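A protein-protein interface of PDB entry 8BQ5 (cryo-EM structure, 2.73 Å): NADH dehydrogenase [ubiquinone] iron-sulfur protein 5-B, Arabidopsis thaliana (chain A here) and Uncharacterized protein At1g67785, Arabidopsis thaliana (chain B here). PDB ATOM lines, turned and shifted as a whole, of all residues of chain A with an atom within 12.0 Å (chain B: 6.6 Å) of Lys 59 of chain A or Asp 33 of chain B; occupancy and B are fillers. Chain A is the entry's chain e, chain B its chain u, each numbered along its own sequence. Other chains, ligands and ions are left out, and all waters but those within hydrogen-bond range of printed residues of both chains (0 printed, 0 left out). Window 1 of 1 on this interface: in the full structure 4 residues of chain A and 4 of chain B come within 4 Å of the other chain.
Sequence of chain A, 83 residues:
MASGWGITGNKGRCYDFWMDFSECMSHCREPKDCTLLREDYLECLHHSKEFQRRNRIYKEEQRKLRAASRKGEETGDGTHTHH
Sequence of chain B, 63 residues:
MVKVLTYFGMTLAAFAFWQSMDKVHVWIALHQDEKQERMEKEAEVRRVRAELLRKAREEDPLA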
ATOM      1  N   SER A  48      17.453  -2.349 -26.695  1.00  0.00           N
ATOM      2  CA  SER A  48      16.293  -2.692 -25.880  1.00  0.00           C
ATOM      3  C   SER A  48      15.381  -1.488 -25.665  1.00  0.00           C
ATOM      4  O   SER A  48      14.157  -1.589 -25.814  1.00  0.00           O
ATOM      5  CB  SER A  48      16.751  -3.274 -24.544  1.00  0.00           C
ATOM      6  OG  SER A  48      15.639  -3.570 -23.721  1.00  0.00           O
ATOM      7  N   LYS A  49      15.957  -0.333 -25.325  1.00  0.00           N
ATOM      8  CA  LYS A  49      15.131   0.830 -25.017  1.00  0.00           C
ATOM      9  C   LYS A  49      14.520   1.436 -26.275  1.00  0.00           C
ATOM     10  O   LYS A  49      13.370   1.893 -26.253  1.00  0.00           O
ATOM     11  CB  LYS A  49      15.949   1.866 -24.250  1.00  0.00           C
ATOM     12  CG  LYS A  49      16.291   1.424 -22.837  1.00  0.00           C
ATOM     13  CD  LYS A  49      17.136   2.449 -22.104  1.00  0.00           C
ATOM     14  CE  LYS A  49      18.227   3.015 -22.986  1.00  0.00           C
ATOM     15  NZ  LYS A  49      19.492   2.251 -22.827  1.00  0.00           N
ATOM     16  N   GLU A  50      15.266   1.446 -27.378  1.00  0.00           N
ATOM     17  CA  GLU A  50      14.709   1.910 -28.645  1.00  0.00           C
ATOM     18  C   GLU A  50      13.492   1.083 -29.041  1.00  0.00           C
ATOM     19  O   GLU A  50      12.428   1.629 -29.369  1.00  0.00           O
ATOM     20  CB  GLU A  50      15.784   1.848 -29.729  1.00  0.00           C
ATOM     21  CG  GLU A  50      15.301   2.218 -31.115  1.00  0.00           C
ATOM     22  CD  GLU A  50      16.403   2.150 -32.152  1.00  0.00           C
ATOM     23  OE1 GLU A  50      16.116   2.389 -33.342  1.00  0.00           O
ATOM     24  OE2 GLU A  50      17.559   1.863 -31.776  1.00  0.00           O
ATOM     25  N   PHE A  51      13.624  -0.243 -28.992  1.00  0.00           N
ATOM     26  CA  PHE A  51      12.515  -1.111 -29.364  1.00  0.00           C
ATOM     27  C   PHE A  51      11.359  -0.981 -28.382  1.00  0.00           C
ATOM     28  O   PHE A  51      10.194  -1.039 -28.782  1.00  0.00           O
ATOM     29  CB  PHE A  51      12.984  -2.563 -29.457  1.00  0.00           C
ATOM     30  CG  PHE A  51      13.870  -2.841 -30.636  1.00  0.00           C
ATOM     31  CD1 PHE A  51      14.014  -1.910 -31.651  1.00  0.00           C
ATOM     32  CD2 PHE A  51      14.560  -4.036 -30.729  1.00  0.00           C
ATOM     33  CE1 PHE A  51      14.830  -2.168 -32.731  1.00  0.00           C
ATOM     34  CE2 PHE A  51      15.375  -4.299 -31.809  1.00  0.00           C
ATOM     35  CZ  PHE A  51      15.511  -3.364 -32.810  1.00  0.00           C
ATOM     36  N   GLN A  52      11.658  -0.805 -27.092  1.00  0.00           N
ATOM     37  CA  GLN A  52      10.593  -0.626 -26.110  1.00  0.00           C
ATOM     38  C   GLN A  52       9.796   0.647 -26.375  1.00  0.00           C
ATOM     39  O   GLN A  52       8.561   0.646 -26.301  1.00  0.00           O
ATOM     40  CB  GLN A  52      11.176  -0.598 -24.700  1.00  0.00           C
ATOM     41  CG  GLN A  52      10.123  -0.604 -23.610  1.00  0.00           C
ATOM     42  CD  GLN A  52      10.579  -1.329 -22.366  1.00  0.00           C
ATOM     43  OE1 GLN A  52      11.633  -1.959 -22.355  1.00  0.00           O
ATOM     44  NE2 GLN A  52       9.784  -1.246 -21.307  1.00  0.00           N
ATOM     45  N   ARG A  53      10.486   1.747 -26.683  1.00  0.00           N
ATOM     46  CA  ARG A  53       9.791   2.998 -26.964  1.00  0.00           C
ATOM     47  C   ARG A  53       8.963   2.896 -28.241  1.00  0.00           C
ATOM     48  O   ARG A  53       7.817   3.371 -28.294  1.00  0.00           O
ATOM     49  CB  ARG A  53      10.806   4.137 -27.050  1.00  0.00           C
ATOM     50  CG  ARG A  53      10.383   5.315 -27.899  1.00  0.00           C
ATOM     51  CD  ARG A  53      11.522   6.313 -28.019  1.00  0.00           C
ATOM     52  NE  ARG A  53      11.104   7.563 -28.641  1.00  0.00           N
ATOM     53  CZ  ARG A  53      10.751   8.651 -27.971  1.00  0.00           C
ATOM     54  NH1 ARG A  53      10.727   8.673 -26.649  1.00  0.00           N
ATOM     55  NH2 ARG A  53      10.414   9.747 -28.646  1.00  0.00           N
ATOM     56  N   ARG A  54       9.516   2.264 -29.281  1.00  0.00           N
ATOM     57  CA  ARG A  54       8.739   2.083 -30.503  1.00  0.00           C
ATOM     58  C   ARG A  54       7.536   1.176 -30.275  1.00  0.00           C
ATOM     59  O   ARG A  54       6.476   1.386 -30.876  1.00  0.00           O
ATOM     60  CB  ARG A  54       9.631   1.541 -31.619  1.00  0.00           C
ATOM     61  CG  ARG A  54      10.490   2.614 -32.267  1.00  0.00           C
ATOM     62  CD  ARG A  54      11.762   2.051 -32.876  1.00  0.00           C
ATOM     63  NE  ARG A  54      11.582   1.651 -34.266  1.00  0.00           N
ATOM     64  CZ  ARG A  54      12.574   1.351 -35.092  1.00  0.00           C
ATOM     65  NH1 ARG A  54      13.839   1.439 -34.715  1.00  0.00           N
ATOM     66  NH2 ARG A  54      12.292   0.955 -36.330  1.00  0.00           N
ATOM     67  N   ASN A  55       7.669   0.175 -29.403  1.00  0.00           N
ATOM     68  CA  ASN A  55       6.522  -0.653 -29.059  1.00  0.00           C
ATOM     69  C   ASN A  55       5.480   0.134 -28.279  1.00  0.00           C
ATOM     70  O   ASN A  55       4.282  -0.120 -28.425  1.00  0.00           O
ATOM     71  CB  ASN A  55       6.976  -1.879 -28.269  1.00  0.00           C
ATOM     72  CG  ASN A  55       7.733  -2.873 -29.125  1.00  0.00           C
ATOM     73  OD1 ASN A  55       7.709  -2.793 -30.353  1.00  0.00           O
ATOM     74  ND2 ASN A  55       8.410  -3.814 -28.484  1.00  0.00           N
ATOM     75  N   ARG A  56       5.912   1.084 -27.446  1.00  0.00           N
ATOM     76  CA  ARG A  56       4.966   2.000 -26.810  1.00  0.00           C
ATOM     77  C   ARG A  56       4.182   2.786 -27.852  1.00  0.00           C
ATOM     78  O   ARG A  56       2.957   2.946 -27.741  1.00  0.00           O
ATOM     79  CB  ARG A  56       5.706   2.962 -25.882  1.00  0.00           C
ATOM     80  CG  ARG A  56       5.568   2.647 -24.413  1.00  0.00           C
ATOM     81  CD  ARG A  56       6.225   3.706 -23.548  1.00  0.00           C
ATOM     82  NE  ARG A  56       7.656   3.806 -23.804  1.00  0.00           N
ATOM     83  CZ  ARG A  56       8.582   3.098 -23.171  1.00  0.00           C
ATOM     84  NH1 ARG A  56       8.259   2.208 -22.246  1.00  0.00           N
ATOM     85  NH2 ARG A  56       9.861   3.283 -23.477  1.00  0.00           N
ATOM     86  N   ILE A  57       4.880   3.293 -28.867  1.00  0.00           N
ATOM     87  CA  ILE A  57       4.216   4.044 -29.933  1.00  0.00           C
ATOM     88  C   ILE A  57       3.195   3.159 -30.644  1.00  0.00           C
ATOM     89  O   ILE A  57       2.051   3.567 -30.895  1.00  0.00           O
ATOM     90  CB  ILE A  57       5.263   4.608 -30.910  1.00  0.00           C
ATOM     91  CG1 ILE A  57       5.802   5.940 -30.391  1.00  0.00           C
ATOM     92  CG2 ILE A  57       4.672   4.778 -32.300  1.00  0.00           C
ATOM     93  CD1 ILE A  57       7.263   6.157 -30.680  1.00  0.00           C
ATOM     94  N   TYR A  58       3.596   1.924 -30.958  1.00  0.00           N
ATOM     95  CA  TYR A  58       2.693   0.969 -31.596  1.00  0.00           C
ATOM     96  C   TYR A  58       1.478   0.680 -30.721  1.00  0.00           C
ATOM     97  O   TYR A  58       0.351   0.579 -31.222  1.00  0.00           O
ATOM     98  CB  TYR A  58       3.458  -0.321 -31.903  1.00  0.00           C
ATOM     99  CG  TYR A  58       2.613  -1.571 -32.025  1.00  0.00           C
ATOM    100  CD1 TYR A  58       2.084  -1.964 -33.247  1.00  0.00           C
ATOM    101  CD2 TYR A  58       2.351  -2.365 -30.914  1.00  0.00           C
ATOM    102  CE1 TYR A  58       1.319  -3.112 -33.357  1.00  0.00           C
ATOM    103  CE2 TYR A  58       1.583  -3.506 -31.014  1.00  0.00           C
ATOM    104  CZ  TYR A  58       1.073  -3.878 -32.234  1.00  0.00           C
ATOM    105  OH  TYR A  58       0.312  -5.020 -32.326  1.00  0.00           O
ATOM    106  N   LYS A  59       1.694   0.522 -29.414  1.00  0.00           N
ATOM    107  CA  LYS A  59       0.599   0.235 -28.494  1.00  0.00           C
ATOM    108  C   LYS A  59      -0.400   1.381 -28.456  1.00  0.00           C
ATOM    109  O   LYS A  59      -1.616   1.160 -28.467  1.00  0.00           O
ATOM    110  CB  LYS A  59       1.147  -0.029 -27.091  1.00  0.00           C
ATOM    111  CG  LYS A  59       0.207  -0.830 -26.204  1.00  0.00           C
ATOM    112  CD  LYS A  59       0.900  -1.381 -24.964  1.00  0.00           C
ATOM    113  CE  LYS A  59       2.388  -1.599 -25.179  1.00  0.00           C
ATOM    114  NZ  LYS A  59       2.987  -2.343 -24.038  1.00  0.00           N
ATOM    115  N   GLU A  60       0.096   2.618 -28.392  1.00  0.00           N
ATOM    116  CA  GLU A  60      -0.810   3.761 -28.374  1.00  0.00           C
ATOM    117  C   GLU A  60      -1.582   3.872 -29.682  1.00  0.00           C
ATOM    118  O   GLU A  60      -2.782   4.182 -29.683  1.00  0.00           O
ATOM    119  CB  GLU A  60      -0.041   5.047 -28.086  1.00  0.00           C
ATOM    120  CG  GLU A  60      -0.920   6.283 -28.089  1.00  0.00           C
ATOM    121  CD  GLU A  60      -1.785   6.387 -26.848  1.00  0.00           C
ATOM    122  OE1 GLU A  60      -1.305   6.044 -25.748  1.00  0.00           O
ATOM    123  OE2 GLU A  60      -2.955   6.804 -26.979  1.00  0.00           O
ATOM    124  N   GLU A  61      -0.914   3.618 -30.810  1.00  0.00           N
ATOM    125  CA  GLU A  61      -1.614   3.644 -32.090  1.00  0.00           C
ATOM    126  C   GLU A  61      -2.716   2.592 -32.133  1.00  0.00           C
ATOM    127  O   GLU A  61      -3.839   2.874 -32.567  1.00  0.00           O
ATOM    128  CB  GLU A  61      -0.623   3.435 -33.233  1.00  0.00           C
ATOM    129  CG  GLU A  61      -1.182   3.741 -34.607  1.00  0.00           C
ATOM    130  CD  GLU A  61      -0.452   2.994 -35.701  1.00  0.00           C
ATOM    131  OE1 GLU A  61       0.086   1.904 -35.415  1.00  0.00           O
ATOM    132  OE2 GLU A  61      -0.403   3.498 -36.842  1.00  0.00           O
ATOM    133  N   GLN A  62      -2.417   1.374 -31.671  1.00  0.00           N
ATOM    134  CA  GLN A  62      -3.427   0.321 -31.630  1.00  0.00           C
ATOM    135  C   GLN A  62      -4.582   0.679 -30.703  1.00  0.00           C
ATOM    136  O   GLN A  62      -5.741   0.392 -31.021  1.00  0.00           O
ATOM    137  CB  GLN A  62      -2.792  -0.999 -31.193  1.00  0.00           C
ATOM    138  CG  GLN A  62      -3.227  -2.220 -31.991  1.00  0.00           C
ATOM    139  CD  GLN A  62      -2.934  -2.109 -33.476  1.00  0.00           C
ATOM    140  OE1 GLN A  62      -2.083  -1.327 -33.902  1.00  0.00           O
ATOM    141  NE2 GLN A  62      -3.629  -2.911 -34.273  1.00  0.00           N
ATOM    142  N   ARG A  63      -4.285   1.286 -29.552  1.00  0.00           N
ATOM    143  CA  ARG A  63      -5.340   1.694 -28.631  1.00  0.00           C
ATOM    144  C   ARG A  63      -6.253   2.737 -29.260  1.00  0.00           C
ATOM    145  O   ARG A  63      -7.479   2.666 -29.112  1.00  0.00           O
ATOM    146  CB  ARG A  63      -4.727   2.229 -27.337  1.00  0.00           C
ATOM    147  CG  ARG A  63      -5.743   2.497 -26.247  1.00  0.00           C
ATOM    148  CD  ARG A  63      -5.156   3.325 -25.116  1.00  0.00           C
ATOM    149  NE  ARG A  63      -4.766   4.666 -25.533  1.00  0.00           N
ATOM    150  CZ  ARG A  63      -5.609   5.679 -25.690  1.00  0.00           C
ATOM    151  NH1 ARG A  63      -6.915   5.519 -25.552  1.00  0.00           N
ATOM    152  NH2 ARG A  63      -5.129   6.882 -25.989  1.00  0.00           N
ATOM    153  N   LYS A  64      -5.680   3.708 -29.975  1.00  0.00           N
ATOM    154  CA  LYS A  64      -6.459   4.780 -30.584  1.00  0.00           C
ATOM    155  C   LYS A  64      -6.972   4.423 -31.975  1.00  0.00           C
ATOM    156  O   LYS A  64      -7.230   5.322 -32.786  1.00  0.00           O
ATOM    157  CB  LYS A  64      -5.635   6.067 -30.641  1.00  0.00           C
ATOM    158  CG  LYS A  64      -5.398   6.724 -29.291  1.00  0.00           C
ATOM    159  CD  LYS A  64      -4.641   8.036 -29.443  1.00  0.00           C
ATOM    160  CE  LYS A  64      -5.066   9.051 -28.391  1.00  0.00           C
ATOM    161  NZ  LYS A  64      -4.770  10.451 -28.800  1.00  0.00           N
ATOM    162  N   LEU A  65      -7.126   3.139 -32.276  1.00  0.00           N
ATOM    163  CA  LEU A  65      -7.639   2.725 -33.574  1.00  0.00           C
ATOM    164  C   LEU A  65      -8.864   1.830 -33.416  1.00  0.00           C
ATOM    165  O   LEU A  65      -8.750   0.671 -33.019  1.00  0.00           O
ATOM    166  CB  LEU A  65      -6.559   1.997 -34.373  1.00  0.00           C
ATOM    167  CG  LEU A  65      -7.002   1.504 -35.750  1.00  0.00           C
ATOM    168  CD1 LEU A  65      -7.243   2.683 -36.685  1.00  0.00           C
ATOM    169  CD2 LEU A  65      -5.987   0.536 -36.335  1.00  0.00           C
ATOM    170  N   ALA B  29       6.242  -9.200 -25.460  1.00  0.00           N
ATOM    171  CA  ALA B  29       6.699  -7.858 -25.801  1.00  0.00           C
ATOM    172  C   ALA B  29       5.675  -6.803 -25.399  1.00  0.00           C
ATOM    173  O   ALA B  29       6.041  -5.712 -24.948  1.00  0.00           O
ATOM    174  CB  ALA B  29       6.999  -7.765 -27.296  1.00  0.00           C
ATOM    175  N   LEU B  30       4.384  -7.110 -25.554  1.00  0.00           N
ATOM    176  CA  LEU B  30       3.346  -6.122 -25.274  1.00  0.00           C
ATOM    177  C   LEU B  30       3.233  -5.778 -23.792  1.00  0.00           C
ATOM    178  O   LEU B  30       2.664  -4.735 -23.457  1.00  0.00           O
ATOM    179  CB  LEU B  30       1.996  -6.617 -25.792  1.00  0.00           C
ATOM    180  CG  LEU B  30       1.710  -6.356 -27.272  1.00  0.00           C
ATOM    181  CD1 LEU B  30       0.560  -7.219 -27.761  1.00  0.00           C
ATOM    182  CD2 LEU B  30       1.415  -4.885 -27.516  1.00  0.00           C
ATOM    183  N   HIS B  31       3.759  -6.618 -22.902  1.00  0.00           N
ATOM    184  CA  HIS B  31       3.624  -6.421 -21.465  1.00  0.00           C
ATOM    185  C   HIS B  31       4.922  -5.964 -20.810  1.00  0.00           C
ATOM    186  O   HIS B  31       5.111  -6.180 -19.608  1.00  0.00           O
ATOM    187  CB  HIS B  31       3.113  -7.702 -20.811  1.00  0.00           C
ATOM    188  CG  HIS B  31       1.708  -8.043 -21.194  1.00  0.00           C
ATOM    189  ND1 HIS B  31       1.358  -8.403 -22.477  1.00  0.00           N
ATOM    190  CD2 HIS B  31       0.563  -8.060 -20.472  1.00  0.00           C
ATOM    191  CE1 HIS B  31       0.058  -8.635 -22.528  1.00  0.00           C
ATOM    192  NE2 HIS B  31      -0.447  -8.433 -21.325  1.00  0.00           N
ATOM    193  N   GLN B  32       5.822  -5.348 -21.578  1.00  0.00           N
ATOM    194  CA  GLN B  32       7.049  -4.814 -20.998  1.00  0.00           C
ATOM    195  C   GLN B  32       6.759  -3.619 -20.100  1.00  0.00           C
ATOM    196  O   GLN B  32       7.351  -3.477 -19.028  1.00  0.00           O
ATOM    197  CB  GLN B  32       8.024  -4.415 -22.105  1.00  0.00           C
ATOM    198  CG  GLN B  32       8.788  -5.560 -22.743  1.00  0.00           C
ATOM    199  CD  GLN B  32       9.464  -6.449 -21.724  1.00  0.00           C
ATOM    200  OE1 GLN B  32       9.062  -7.592 -21.517  1.00  0.00           O
ATOM    201  NE2 GLN B  32      10.488  -5.920 -21.066  1.00  0.00           N
ATOM    202  N   ASP B  33       5.853  -2.742 -20.523  1.00  0.00           N
ATOM    203  CA  ASP B  33       5.596  -1.533 -19.752  1.00  0.00           C
ATOM    204  C   ASP B  33       4.968  -1.858 -18.402  1.00  0.00           C
ATOM    205  O   ASP B  33       5.361  -1.289 -17.377  1.00  0.00           O
ATOM    206  CB  ASP B  33       4.710  -0.599 -20.564  1.00  0.00           C
ATOM    207  CG  ASP B  33       5.479   0.100 -21.658  1.00  0.00           C
ATOM    208  OD1 ASP B  33       4.987   0.125 -22.805  1.00  0.00           O
ATOM    209  OD2 ASP B  33       6.582   0.611 -21.373  1.00  0.00           O
ATOM    210  N   GLU B  34       4.004  -2.781 -18.380  1.00  0.00           N
ATOM    211  CA  GLU B  34       3.403  -3.199 -17.118  1.00  0.00           C
ATOM    212  C   GLU B  34       4.447  -3.801 -16.189  1.00  0.00           C
ATOM    213  O   GLU B  34       4.440  -3.539 -14.982  1.00  0.00           O
ATOM    214  CB  GLU B  34       2.286  -4.209 -17.379  1.00  0.00           C
ATOM    215  CG  GLU B  34       1.646  -4.099 -18.754  1.00  0.00           C
ATOM    216  CD  GLU B  34       0.743  -2.890 -18.887  1.00  0.00           C
ATOM    217  OE1 GLU B  34       0.847  -2.176 -19.908  1.00  0.00           O
ATOM    218  OE2 GLU B  34      -0.075  -2.657 -17.974  1.00  0.00           O
ATOM    219  N   LYS B  35       5.350  -4.616 -16.736  1.00  0.00           N
ATOM    220  CA  LYS B  35       6.364  -5.261 -15.909  1.00  0.00           C
ATOM    221  C   LYS B  35       7.341  -4.242 -15.332  1.00  0.00           C
ATOM    222  O   LYS B  35       7.701  -4.320 -14.154  1.00  0.00           O
ATOM    223  CB  LYS B  35       7.099  -6.327 -16.719  1.00  0.00           C
ATOM    224  CG  LYS B  35       8.067  -7.166 -15.906  1.00  0.00           C
ATOM    225  CD  LYS B  35       8.167  -8.579 -16.455  1.00  0.00           C
ATOM    226  CE  LYS B  35       9.428  -8.762 -17.281  1.00  0.00           C
ATOM    227  NZ  LYS B  35      10.136 -10.026 -16.939  1.00  0.00           N
ATOM    228  N   GLN B  36       7.781  -3.276 -16.144  1.00  0.00           N
ATOM    229  CA  GLN B  36       8.653  -2.224 -15.621  1.00  0.00           C
ATOM    230  C   GLN B  36       7.939  -1.371 -14.579  1.00  0.00           C
ATOM    231  O   GLN B  36       8.543  -0.971 -13.579  1.00  0.00           O
ATOM    232  CB  GLN B  36       9.189  -1.351 -16.757  1.00  0.00           C
ATOM    233  CG  GLN B  36      10.231  -0.298 -16.358  1.00  0.00           C
ATOM    234  CD  GLN B  36      10.862   0.435 -17.533  1.00  0.00           C
ATOM    235  OE1 GLN B  36      10.613   0.122 -18.684  1.00  0.00           O
ATOM    236  NE2 GLN B  36      11.690   1.420 -17.233  1.00  0.00           N
ATOM    237  N   GLU B  37       6.658  -1.070 -14.800  1.00  0.00           N
ATOM    238  CA  GLU B  37       5.898  -0.299 -13.819  1.00  0.00           C
ATOM    239  C   GLU B  37       5.780  -1.049 -12.497  1.00  0.00           C
ATOM    240  O   GLU B  37       5.949  -0.465 -11.418  1.00  0.00           O
ATOM    241  CB  GLU B  37       4.513   0.019 -14.378  1.00  0.00           C
ATOM    242  CG  GLU B  37       3.699   0.982 -13.540  1.00  0.00           C
ATOM    243  CD  GLU B  37       2.252   1.042 -13.986  1.00  0.00           C
ATOM    244  OE1 GLU B  37       1.853   0.194 -14.812  1.00  0.00           O
ATOM    245  OE2 GLU B  37       1.519   1.935 -13.515  1.00  0.00           O
ATOM    246  N   ARG B  38       5.488  -2.349 -12.567  1.00  0.00           N
ATOM    247  CA  ARG B  38       5.415  -3.168 -11.363  1.00  0.00           C
ATOM    248  C   ARG B  38       6.768  -3.234 -10.665  1.00  0.00           C
ATOM    249  O   ARG B  38       6.849  -3.144  -9.432  1.00  0.00           O
ATOM    250  CB  ARG B  38       4.915  -4.563 -11.737  1.00  0.00           C
ATOM    251  CG  ARG B  38       4.759  -5.533 -10.585  1.00  0.00           C
ATOM    252  CD  ARG B  38       4.189  -6.851 -11.080  1.00  0.00           C
ATOM    253  NE  ARG B  38       3.999  -7.814  -9.998  1.00  0.00           N
ATOM    254  CZ  ARG B  38       3.347  -8.964 -10.111  1.00  0.00           C
ATOM    255  NH1 ARG B  38       2.780  -9.332 -11.248  1.00  0.00           N
ATOM    256  NH2 ARG B  38       3.257  -9.764  -9.051  1.00  0.00           N
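Among the printed residues, merely in contact across the chains: Gln 52 of chain A with Asp 33 of chain B (3.7 Å), Gln 52 of chain A with Gln 32 of chain B (3.7 Å) and Tyr 58 of chain A with Leu 30 of chain B (3.8 Å).
Lys 59 of chain A touches two residues of chain B. Asp 33 of chain B touches three residues of chain A. Of chain A, only Tyr 58 and Lys 59 come within 4 Å of Leu 30 of chain B. Gln 32 of chain B touches one residue of chain A. No residue of chain A comes within 4 Å of Glu 34 of chain B. Gln 36 of chain B touches just one residue of chain A: Gln 52. Glu 37 of chain B touches none of the printed residues of chain A. Of the printed residues of chain B, Arg 56 of chain A touches Asp 33 (2.5 Å). Of the printed residues of chain B, Tyr 58 of chain A touches Leu 30 (3.8 Å). Glu 50 of chain A touches none of the printed residues of chain B. The nearest printed residue of chain B that does not touch Gln 52 of chain A is Glu 34 of chain B (6.7 Å).
Of the 18 printed residues of chain A, 4 touch a printed residue of chain B. Printed residues of chain A that touch a printed residue of chain B: Gln 52, Arg 56, Tyr 58 and Lys 59. Hydrophobic or aromatic side chains of chain A within 4 Å of the printed part of chain B: Tyr 58. Of the 10 printed residues of chain B, 4 touch a printed residue of chain A. Hydrophobic or aromatic side chains of chain B within 4 Å of the printed part of chain A: Leu 30. Among the printed residues, 7 pairs touch across the chains.
The side-chain amide nitrogen (NE2) of Gln 52 of chain A is in hydrogen-bond range of the side-chain amide oxygen (OE1) of Gln 36 of chain B (3.1 Å). The guanidinium group (NH1) of Arg 56 of chain A is in salt-bridge range of the side-chain carboxylate (OD2) of Asp 33 of chain B (2.5 Å). The side-chain amino group (NZ) of Lys 59 of chain A sits at hydrogen-bond distance from the backbone carbonyl oxygen (O) of Leu 30 of chain B, at 2.5 Å. NZ of Lys 59 of chain A is in salt-bridge range of OD1 of Asp 33 of chain B, at 3.4 Å.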
